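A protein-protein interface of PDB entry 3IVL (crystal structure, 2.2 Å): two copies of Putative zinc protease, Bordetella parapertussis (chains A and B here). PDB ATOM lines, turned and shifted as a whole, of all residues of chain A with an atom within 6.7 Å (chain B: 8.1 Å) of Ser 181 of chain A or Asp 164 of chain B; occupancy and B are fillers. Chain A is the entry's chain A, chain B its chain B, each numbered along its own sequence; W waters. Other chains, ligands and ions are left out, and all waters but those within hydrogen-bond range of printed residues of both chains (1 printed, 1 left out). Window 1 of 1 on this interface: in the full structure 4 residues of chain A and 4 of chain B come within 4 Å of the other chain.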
ATOM      1  N   TYR A  28     -40.404   6.651 -24.233  1.00  0.00           N
ATOM      2  CA  TYR A  28     -39.409   6.583 -25.246  1.00  0.00           C
ATOM      3  C   TYR A  28     -40.009   6.122 -26.546  1.00  0.00           C
ATOM      4  O   TYR A  28     -40.769   5.222 -26.561  1.00  0.00           O
ATOM      5  CB  TYR A  28     -38.381   5.611 -24.810  1.00  0.00           C
ATOM      6  CG  TYR A  28     -37.758   5.951 -23.516  1.00  0.00           C
ATOM      7  CD1 TYR A  28     -36.530   6.556 -23.466  1.00  0.00           C
ATOM      8  CD2 TYR A  28     -38.380   5.667 -22.338  1.00  0.00           C
ATOM      9  CE1 TYR A  28     -35.939   6.864 -22.270  1.00  0.00           C
ATOM     10  CE2 TYR A  28     -37.800   5.959 -21.151  1.00  0.00           C
ATOM     11  CZ  TYR A  28     -36.573   6.563 -21.118  1.00  0.00           C
ATOM     12  OH  TYR A  28     -36.010   6.866 -19.950  1.00  0.00           O
ATOM     13  N   GLU A 106     -31.995   4.094 -18.312  1.00  0.00           N
ATOM     14  CA  GLU A 106     -30.995   4.552 -19.241  1.00  0.00           C
ATOM     15  C   GLU A 106     -29.555   4.089 -18.929  1.00  0.00           C
ATOM     16  O   GLU A 106     -28.589   4.537 -19.511  1.00  0.00           O
ATOM     17  CB  GLU A 106     -31.101   6.059 -19.348  1.00  0.00           C
ATOM     18  CG  GLU A 106     -32.458   6.461 -19.802  1.00  0.00           C
ATOM     19  CD  GLU A 106     -32.642   7.916 -19.881  1.00  0.00           C
ATOM     20  OE1 GLU A 106     -31.660   8.624 -19.830  1.00  0.00           O
ATOM     21  OE2 GLU A 106     -33.767   8.375 -20.001  1.00  0.00           O
ATOM     22  N   ALA A 176     -30.063   0.944 -26.954  1.00  0.00           N
ATOM     23  CA  ALA A 176     -30.238   1.922 -28.006  1.00  0.00           C
ATOM     24  C   ALA A 176     -31.385   2.882 -27.907  1.00  0.00           C
ATOM     25  O   ALA A 176     -31.270   4.002 -28.320  1.00  0.00           O
ATOM     26  CB  ALA A 176     -30.263   1.264 -29.322  1.00  0.00           C
ATOM     27  N   TYR A 177     -32.527   2.414 -27.451  1.00  0.00           N
ATOM     28  CA  TYR A 177     -33.699   3.259 -27.407  1.00  0.00           C
ATOM     29  C   TYR A 177     -33.989   3.901 -26.068  1.00  0.00           C
ATOM     30  O   TYR A 177     -34.637   4.893 -26.016  1.00  0.00           O
ATOM     31  CB  TYR A 177     -34.904   2.501 -27.914  1.00  0.00           C
ATOM     32  CG  TYR A 177     -34.848   2.242 -29.371  1.00  0.00           C
ATOM     33  CD1 TYR A 177     -35.445   3.088 -30.253  1.00  0.00           C
ATOM     34  CD2 TYR A 177     -34.171   1.165 -29.870  1.00  0.00           C
ATOM     35  CE1 TYR A 177     -35.379   2.862 -31.572  1.00  0.00           C
ATOM     36  CE2 TYR A 177     -34.103   0.943 -31.194  1.00  0.00           C
ATOM     37  CZ  TYR A 177     -34.711   1.790 -32.029  1.00  0.00           C
ATOM     38  OH  TYR A 177     -34.651   1.595 -33.338  1.00  0.00           O
ATOM     39  N   LEU A 178     -33.515   3.305 -24.994  1.00  0.00           N
ATOM     40  CA  LEU A 178     -33.716   3.870 -23.685  1.00  0.00           C
ATOM     41  C   LEU A 178     -32.623   4.867 -23.376  1.00  0.00           C
ATOM     42  O   LEU A 178     -31.670   4.574 -22.742  1.00  0.00           O
ATOM     43  CB  LEU A 178     -33.776   2.772 -22.648  1.00  0.00           C
ATOM     44  CG  LEU A 178     -34.916   1.802 -22.880  1.00  0.00           C
ATOM     45  CD1 LEU A 178     -34.999   0.801 -21.813  1.00  0.00           C
ATOM     46  CD2 LEU A 178     -36.198   2.534 -23.028  1.00  0.00           C
ATOM     47  N   VAL A 179     -32.805   6.052 -23.887  1.00  0.00           N
ATOM     48  CA  VAL A 179     -31.777   7.026 -23.954  1.00  0.00           C
ATOM     49  C   VAL A 179     -32.386   8.421 -23.821  1.00  0.00           C
ATOM     50  O   VAL A 179     -33.463   8.678 -24.288  1.00  0.00           O
ATOM     51  CB  VAL A 179     -31.030   6.794 -25.274  1.00  0.00           C
ATOM     52  CG1 VAL A 179     -31.486   7.649 -26.368  1.00  0.00           C
ATOM     53  CG2 VAL A 179     -29.612   6.750 -25.104  1.00  0.00           C
ATOM     54  N   ARG A 180     -31.676   9.320 -23.174  1.00  0.00           N
ATOM     55  CA  ARG A 180     -32.179  10.635 -22.837  1.00  0.00           C
ATOM     56  C   ARG A 180     -32.487  11.406 -24.076  1.00  0.00           C
ATOM     57  O   ARG A 180     -33.371  12.226 -24.112  1.00  0.00           O
ATOM     58  CB  ARG A 180     -31.198  11.373 -21.937  1.00  0.00           C
ATOM     59  CG  ARG A 180     -31.643  12.697 -21.410  1.00  0.00           C
ATOM     60  CD  ARG A 180     -30.493  13.317 -20.712  1.00  0.00           C
ATOM     61  NE  ARG A 180     -30.836  14.210 -19.632  1.00  0.00           N
ATOM     62  CZ  ARG A 180     -31.182  15.464 -19.794  1.00  0.00           C
ATOM     63  NH1 ARG A 180     -31.283  15.990 -20.981  1.00  0.00           N
ATOM     64  NH2 ARG A 180     -31.476  16.171 -18.757  1.00  0.00           N
ATOM     65  N   SER A 181     -31.774  11.079 -25.127  1.00  0.00           N
ATOM     66  CA  SER A 181     -32.015  11.671 -26.411  1.00  0.00           C
ATOM     67  C   SER A 181     -33.425  11.361 -26.843  1.00  0.00           C
ATOM     68  O   SER A 181     -34.021  12.137 -27.529  1.00  0.00           O
ATOM     69  CB  SER A 181     -31.027  11.160 -27.459  1.00  0.00           C
ATOM     70  OG  SER A 181     -29.978  10.400 -26.911  1.00  0.00           O
ATOM     71  N   ASN A 182     -33.911  10.194 -26.462  1.00  0.00           N
ATOM     72  CA  ASN A 182     -35.236   9.676 -26.805  1.00  0.00           C
ATOM     73  C   ASN A 182     -36.295   9.859 -25.693  1.00  0.00           C
ATOM     74  O   ASN A 182     -37.416   9.455 -25.827  1.00  0.00           O
ATOM     75  CB  ASN A 182     -35.060   8.189 -27.134  1.00  0.00           C
ATOM     76  CG  ASN A 182     -36.173   7.590 -27.984  1.00  0.00           C
ATOM     77  OD1 ASN A 182     -36.823   8.241 -28.756  1.00  0.00           O
ATOM     78  ND2 ASN A 182     -36.364   6.329 -27.819  1.00  0.00           N
ATOM     79  N   ARG A 183     -35.919  10.451 -24.579  1.00  0.00           N
ATOM     80  CA  ARG A 183     -36.812  10.576 -23.443  1.00  0.00           C
ATOM     81  C   ARG A 183     -37.831  11.702 -23.463  1.00  0.00           C
ATOM     82  O   ARG A 183     -37.522  12.817 -23.755  1.00  0.00           O
ATOM     83  CB  ARG A 183     -36.007  10.624 -22.184  1.00  0.00           C
ATOM     84  CG  ARG A 183     -36.799  10.505 -20.956  1.00  0.00           C
ATOM     85  CD  ARG A 183     -36.191  11.257 -19.801  1.00  0.00           C
ATOM     86  NE  ARG A 183     -34.877  10.775 -19.463  1.00  0.00           N
ATOM     87  CZ  ARG A 183     -34.011  11.446 -18.738  1.00  0.00           C
ATOM     88  NH1 ARG A 183     -34.326  12.622 -18.266  1.00  0.00           N
ATOM     89  NH2 ARG A 183     -32.846  10.935 -18.488  1.00  0.00           N
ATOM     90  N   VAL B  39     -19.021  18.326 -30.484  1.00  0.00           N
ATOM     91  CA  VAL B  39     -19.153  17.481 -29.327  1.00  0.00           C
ATOM     92  C   VAL B  39     -19.031  16.024 -29.719  1.00  0.00           C
ATOM     93  O   VAL B  39     -18.436  15.260 -29.047  1.00  0.00           O
ATOM     94  CB  VAL B  39     -20.434  17.796 -28.561  1.00  0.00           C
ATOM     95  CG1 VAL B  39     -20.926  16.622 -27.865  1.00  0.00           C
ATOM     96  CG2 VAL B  39     -20.199  18.887 -27.590  1.00  0.00           C
ATOM     97  N   LEU B  43     -16.219  13.356 -28.295  1.00  0.00           N
ATOM     98  CA  LEU B  43     -16.533  12.006 -27.838  1.00  0.00           C
ATOM     99  C   LEU B  43     -15.880  10.887 -28.669  1.00  0.00           C
ATOM    100  O   LEU B  43     -15.329   9.983 -28.118  1.00  0.00           O
ATOM    101  CB  LEU B  43     -18.043  11.796 -27.672  1.00  0.00           C
ATOM    102  CG  LEU B  43     -18.850  12.682 -26.736  1.00  0.00           C
ATOM    103  CD1 LEU B  43     -20.259  12.585 -27.013  1.00  0.00           C
ATOM    104  CD2 LEU B  43     -18.563  12.480 -25.337  1.00  0.00           C
ATOM    105  N   GLN B 115     -22.937   1.560 -28.734  1.00  0.00           N
ATOM    106  CA  GLN B 115     -23.515   2.382 -27.674  1.00  0.00           C
ATOM    107  C   GLN B 115     -22.708   2.213 -26.441  1.00  0.00           C
ATOM    108  O   GLN B 115     -22.604   3.094 -25.646  1.00  0.00           O
ATOM    109  CB  GLN B 115     -24.963   2.049 -27.334  1.00  0.00           C
ATOM    110  CG  GLN B 115     -26.022   2.557 -28.281  1.00  0.00           C
ATOM    111  CD  GLN B 115     -26.498   3.955 -28.001  1.00  0.00           C
ATOM    112  OE1 GLN B 115     -26.046   4.625 -27.093  1.00  0.00           O
ATOM    113  NE2 GLN B 115     -27.433   4.396 -28.803  1.00  0.00           N
ATOM    114  N   LEU B 118     -19.862   4.613 -26.528  1.00  0.00           N
ATOM    115  CA  LEU B 118     -20.355   5.957 -26.371  1.00  0.00           C
ATOM    116  C   LEU B 118     -20.757   6.374 -24.971  1.00  0.00           C
ATOM    117  O   LEU B 118     -20.453   7.464 -24.541  1.00  0.00           O
ATOM    118  CB  LEU B 118     -21.543   6.131 -27.274  1.00  0.00           C
ATOM    119  CG  LEU B 118     -21.898   7.575 -27.514  1.00  0.00           C
ATOM    120  CD1 LEU B 118     -23.335   7.788 -27.411  1.00  0.00           C
ATOM    121  CD2 LEU B 118     -21.183   8.370 -26.520  1.00  0.00           C
ATOM    122  N   GLU B 119     -21.467   5.507 -24.273  1.00  0.00           N
ATOM    123  CA  GLU B 119     -21.836   5.760 -22.895  1.00  0.00           C
ATOM    124  C   GLU B 119     -20.652   5.812 -21.980  1.00  0.00           C
ATOM    125  O   GLU B 119     -20.620   6.586 -21.078  1.00  0.00           O
ATOM    126  CB  GLU B 119     -22.877   4.775 -22.403  1.00  0.00           C
ATOM    127  CG  GLU B 119     -24.167   4.893 -23.097  1.00  0.00           C
ATOM    128  CD  GLU B 119     -24.983   6.061 -22.620  1.00  0.00           C
ATOM    129  OE1 GLU B 119     -24.598   6.730 -21.660  1.00  0.00           O
ATOM    130  OE2 GLU B 119     -26.023   6.299 -23.222  1.00  0.00           O
ATOM    131  N   ARG B 122     -19.224   9.242 -22.888  1.00  0.00           N
ATOM    132  CA  ARG B 122     -19.989  10.346 -22.423  1.00  0.00           C
ATOM    133  C   ARG B 122     -19.821  10.522 -20.955  1.00  0.00           C
ATOM    134  O   ARG B 122     -19.715  11.624 -20.480  1.00  0.00           O
ATOM    135  CB  ARG B 122     -21.429  10.131 -22.747  1.00  0.00           C
ATOM    136  CG  ARG B 122     -22.327  10.881 -21.873  1.00  0.00           C
ATOM    137  CD  ARG B 122     -23.697  10.405 -22.071  1.00  0.00           C
ATOM    138  NE  ARG B 122     -24.170  10.861 -23.342  1.00  0.00           N
ATOM    139  CZ  ARG B 122     -24.736  10.102 -24.244  1.00  0.00           C
ATOM    140  NH1 ARG B 122     -24.918   8.835 -24.006  1.00  0.00           N
ATOM    141  NH2 ARG B 122     -25.130  10.614 -25.371  1.00  0.00           N
ATOM    142  N   LEU B 126     -18.442  13.947 -18.990  1.00  0.00           N
ATOM    143  CA  LEU B 126     -19.245  14.572 -17.973  1.00  0.00           C
ATOM    144  C   LEU B 126     -18.588  14.539 -16.617  1.00  0.00           C
ATOM    145  O   LEU B 126     -18.746  15.423 -15.847  1.00  0.00           O
ATOM    146  CB  LEU B 126     -20.642  14.020 -17.945  1.00  0.00           C
ATOM    147  CG  LEU B 126     -21.471  14.234 -19.186  1.00  0.00           C
ATOM    148  CD1 LEU B 126     -22.678  13.485 -19.076  1.00  0.00           C
ATOM    149  CD2 LEU B 126     -21.781  15.653 -19.530  1.00  0.00           C
ATOM    150  N   LEU B 157     -23.297  24.808 -22.572  1.00  0.00           N
ATOM    151  CA  LEU B 157     -23.881  24.195 -23.728  1.00  0.00           C
ATOM    152  C   LEU B 157     -23.229  22.884 -24.128  1.00  0.00           C
ATOM    153  O   LEU B 157     -23.894  21.988 -24.541  1.00  0.00           O
ATOM    154  CB  LEU B 157     -23.914  25.134 -24.912  1.00  0.00           C
ATOM    155  CG  LEU B 157     -24.594  26.469 -24.808  1.00  0.00           C
ATOM    156  CD1 LEU B 157     -24.473  27.181 -26.078  1.00  0.00           C
ATOM    157  CD2 LEU B 157     -25.997  26.285 -24.494  1.00  0.00           C
ATOM    158  N   GLN B 158     -21.929  22.772 -24.001  1.00  0.00           N
ATOM    159  CA  GLN B 158     -21.284  21.530 -24.338  1.00  0.00           C
ATOM    160  C   GLN B 158     -21.719  20.381 -23.438  1.00  0.00           C
ATOM    161  O   GLN B 158     -21.922  19.305 -23.898  1.00  0.00           O
ATOM    162  CB  GLN B 158     -19.769  21.631 -24.423  1.00  0.00           C
ATOM    163  CG  GLN B 158     -19.248  22.866 -25.054  1.00  0.00           C
ATOM    164  CD  GLN B 158     -18.879  22.706 -26.480  1.00  0.00           C
ATOM    165  OE1 GLN B 158     -19.714  22.540 -27.322  1.00  0.00           O
ATOM    166  NE2 GLN B 158     -17.615  22.791 -26.758  1.00  0.00           N
ATOM    167  N   ARG B 159     -21.893  20.653 -22.164  1.00  0.00           N
ATOM    168  CA  ARG B 159     -22.398  19.654 -21.262  1.00  0.00           C
ATOM    169  C   ARG B 159     -23.767  19.191 -21.683  1.00  0.00           C
ATOM    170  O   ARG B 159     -24.020  18.034 -21.707  1.00  0.00           O
ATOM    171  CB  ARG B 159     -22.466  20.211 -19.861  1.00  0.00           C
ATOM    172  CG  ARG B 159     -22.872  19.237 -18.770  1.00  0.00           C
ATOM    173  CD  ARG B 159     -24.355  19.203 -18.600  1.00  0.00           C
ATOM    174  NE  ARG B 159     -24.941  20.508 -18.823  1.00  0.00           N
ATOM    175  CZ  ARG B 159     -25.196  21.363 -17.856  1.00  0.00           C
ATOM    176  NH1 ARG B 159     -24.947  21.042 -16.617  1.00  0.00           N
ATOM    177  NH2 ARG B 159     -25.682  22.540 -18.128  1.00  0.00           N
ATOM    178  N   ASP B 160     -24.638  20.105 -22.047  1.00  0.00           N
ATOM    179  CA  ASP B 160     -25.954  19.729 -22.490  1.00  0.00           C
ATOM    180  C   ASP B 160     -25.894  18.888 -23.750  1.00  0.00           C
ATOM    181  O   ASP B 160     -26.602  17.930 -23.895  1.00  0.00           O
ATOM    182  CB  ASP B 160     -26.812  20.954 -22.774  1.00  0.00           C
ATOM    183  CG  ASP B 160     -27.201  21.718 -21.538  1.00  0.00           C
ATOM    184  OD1 ASP B 160     -26.973  21.291 -20.419  1.00  0.00           O
ATOM    185  OD2 ASP B 160     -27.714  22.801 -21.701  1.00  0.00           O
ATOM    186  N   ARG B 161     -25.048  19.294 -24.673  1.00  0.00           N
ATOM    187  CA  ARG B 161     -24.838  18.580 -25.896  1.00  0.00           C
ATOM    188  C   ARG B 161     -24.256  17.199 -25.683  1.00  0.00           C
ATOM    189  O   ARG B 161     -24.603  16.311 -26.364  1.00  0.00           O
ATOM    190  CB  ARG B 161     -23.998  19.389 -26.850  1.00  0.00           C
ATOM    191  CG  ARG B 161     -24.734  20.477 -27.554  1.00  0.00           C
ATOM    192  CD  ARG B 161     -23.815  21.580 -27.955  1.00  0.00           C
ATOM    193  NE  ARG B 161     -24.561  22.764 -28.294  1.00  0.00           N
ATOM    194  CZ  ARG B 161     -24.079  23.792 -28.942  1.00  0.00           C
ATOM    195  NH1 ARG B 161     -22.848  23.801 -29.328  1.00  0.00           N
ATOM    196  NH2 ARG B 161     -24.844  24.803 -29.201  1.00  0.00           N
ATOM    197  N   VAL B 162     -23.362  17.037 -24.746  1.00  0.00           N
ATOM    198  CA  VAL B 162     -22.816  15.743 -24.463  1.00  0.00           C
ATOM    199  C   VAL B 162     -23.880  14.775 -23.948  1.00  0.00           C
ATOM    200  O   VAL B 162     -23.929  13.646 -24.357  1.00  0.00           O
ATOM    201  CB  VAL B 162     -21.600  15.855 -23.591  1.00  0.00           C
ATOM    202  CG1 VAL B 162     -21.238  14.574 -23.001  1.00  0.00           C
ATOM    203  CG2 VAL B 162     -20.473  16.346 -24.392  1.00  0.00           C
ATOM    204  N   ARG B 163     -24.760  15.240 -23.081  1.00  0.00           N
ATOM    205  CA  ARG B 163     -25.861  14.431 -22.607  1.00  0.00           C
ATOM    206  C   ARG B 163     -26.823  14.027 -23.687  1.00  0.00           C
ATOM    207  O   ARG B 163     -27.327  12.974 -23.648  1.00  0.00           O
ATOM    208  CB  ARG B 163     -26.680  15.151 -21.578  1.00  0.00           C
ATOM    209  CG  ARG B 163     -26.029  15.447 -20.341  1.00  0.00           C
ATOM    210  CD  ARG B 163     -26.441  16.821 -20.056  1.00  0.00           C
ATOM    211  NE  ARG B 163     -27.144  16.950 -18.805  1.00  0.00           N
ATOM    212  CZ  ARG B 163     -28.112  17.812 -18.586  1.00  0.00           C
ATOM    213  NH1 ARG B 163     -28.567  18.594 -19.535  1.00  0.00           N
ATOM    214  NH2 ARG B 163     -28.638  17.849 -17.403  1.00  0.00           N
ATOM    215  N   ASP B 164     -27.114  14.901 -24.615  1.00  0.00           N
ATOM    216  CA  ASP B 164     -28.087  14.609 -25.638  1.00  0.00           C
ATOM    217  C   ASP B 164     -27.546  14.028 -26.935  1.00  0.00           C
ATOM    218  O   ASP B 164     -28.310  13.812 -27.855  1.00  0.00           O
ATOM    219  CB  ASP B 164     -28.895  15.849 -25.971  1.00  0.00           C
ATOM    220  CG  ASP B 164     -29.809  16.294 -24.831  1.00  0.00           C
ATOM    221  OD1 ASP B 164     -30.069  15.525 -23.888  1.00  0.00           O
ATOM    222  OD2 ASP B 164     -30.269  17.440 -24.889  1.00  0.00           O
ATOM    223  N   ALA B 165     -26.244  13.791 -27.010  1.00  0.00           N
ATOM    224  CA  ALA B 165     -25.638  13.406 -28.264  1.00  0.00           C
ATOM    225  C   ALA B 165     -26.057  12.016 -28.636  1.00  0.00           C
ATOM    226  O   ALA B 165     -25.900  11.113 -27.869  1.00  0.00           O
ATOM    227  CB  ALA B 165     -24.172  13.469 -28.149  1.00  0.00           C
ATOM    228  N   LYS B 166     -26.598  11.874 -29.822  1.00  0.00           N
ATOM    229  CA  LYS B 166     -26.989  10.569 -30.332  1.00  0.00           C
ATOM    230  C   LYS B 166     -25.830   9.847 -30.968  1.00  0.00           C
ATOM    231  O   LYS B 166     -25.016  10.435 -31.597  1.00  0.00           O
ATOM    232  CB  LYS B 166     -28.141  10.682 -31.323  1.00  0.00           C
ATOM    233  CG  LYS B 166     -29.258  11.593 -30.869  1.00  0.00           C
ATOM    234  CD  LYS B 166     -30.491  11.421 -31.664  1.00  0.00           C
ATOM    235  CE  LYS B 166     -31.059  12.724 -32.082  1.00  0.00           C
ATOM    236  NZ  LYS B 166     -32.402  12.961 -31.557  1.00  0.00           N
ATOM    237  N   LEU B 167     -25.815   8.545 -30.857  1.00  0.00           N
ATOM    238  CA  LEU B 167     -24.751   7.742 -31.392  1.00  0.00           C
ATOM    239  C   LEU B 167     -24.648   7.928 -32.864  1.00  0.00           C
ATOM    240  O   LEU B 167     -23.589   7.969 -33.391  1.00  0.00           O
ATOM    241  CB  LEU B 167     -24.974   6.275 -31.076  1.00  0.00           C
ATOM    242  CG  LEU B 167     -24.080   5.277 -31.773  1.00  0.00           C
ATOM    243  CD1 LEU B 167     -22.801   5.261 -31.062  1.00  0.00           C
ATOM    244  CD2 LEU B 167     -24.685   3.927 -31.770  1.00  0.00           C
ATOM    245  N   ASP B 169     -25.213  10.605 -34.513  1.00  0.00           N
ATOM    246  CA  ASP B 169     -24.543  11.868 -34.743  1.00  0.00           C
ATOM    247  C   ASP B 169     -23.050  11.814 -34.484  1.00  0.00           C
ATOM    248  O   ASP B 169     -22.283  12.414 -35.174  1.00  0.00           O
ATOM    249  CB  ASP B 169     -25.215  12.985 -33.974  1.00  0.00           C
ATOM    250  CG  ASP B 169     -26.597  13.280 -34.485  1.00  0.00           C
ATOM    251  OD1 ASP B 169     -26.832  13.119 -35.687  1.00  0.00           O
ATOM    252  OD2 ASP B 169     -27.450  13.664 -33.681  1.00  0.00           O
ATOM    253  N   VAL B 170     -22.657  11.111 -33.448  1.00  0.00           N
ATOM    254  CA  VAL B 170     -21.273  10.927 -33.182  1.00  0.00           C
ATOM    255  C   VAL B 170     -20.633  10.152 -34.296  1.00  0.00           C
ATOM    256  O   VAL B 170     -19.584  10.488 -34.746  1.00  0.00           O
ATOM    257  CB  VAL B 170     -21.074  10.160 -31.944  1.00  0.00           C
ATOM    258  CG1 VAL B 170     -19.670   9.884 -31.748  1.00  0.00           C
ATOM    259  CG2 VAL B 170     -21.596  10.892 -30.801  1.00  0.00           C
HETATM  260  O   HOH W   1     -28.638  10.499 -24.337  1.00  0.00           O
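Printed residues of chain A that touch a printed residue of chain B: Ala 176, Arg 180 and Ser 181.
Of the 20 printed residues of chain B, 4 touch a printed residue of chain A.
OD1 of Asp 164 of chain B lies within salt-bridge range of NH1 of Arg 180 of chain A (3.2 Å).
OD1 of Asp 160 of chain B is in salt-bridge range of NH1 of Arg 163 of chain B.
The side-chain carboxylate (OE1) of Glu 106 of chain A sits at hydrogen-bond distance from the backbone NH (N) of Arg 180 of chain A, 3.4 Å away.
Of chain B, only Asp 164 (3.8 Å) and Lys 166 (3.9 Å) come within 4 Å of Ser 181 of chain A.
Of chain A, only Arg 180 (3.2 Å) and Ser 181 (3.8 Å) come within 4 Å of Asp 164 of chain B.
Of the printed residues of chain A, Lys 166 of chain B touches Ser 181.
Of the printed residues of chain B, Arg 180 of chain A touches Arg 163 (3.6 Å) and Asp 164 (3.2 Å).
Printed residues of chain A within 4 Å of Arg 163 of chain B: Arg 180.
Printed residues of chain B within 4 Å of Ala 176 of chain A: Gln 115 (3.8 Å).
The nearest printed residue of chain A that does not touch Asp 164 of chain B is Asn 182 of chain A (6.8 Å).
Ala 176 of chain A touches Gln 115 of chain B (CA to NE2, 3.8 Å).
Arg 180 of chain A touches Arg 163 of chain B (NH2 to NH2, 3.6 Å).
Asp 164 of chain B touches Ser 181 of chain A.
Ser 181 of chain A touches Lys 166 of chain B (CB to CG, 3.9 Å).
No position is printed for both chains.
Of the 5 pairs that touch across the chains among the printed residues, none has its exchanged pair printed and touching as well.
Water W1 lies within hydrogen-bond range of O of Arg 163 of chain B, OG of Ser 181 of chain A and N of Arg 180 of chain A.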
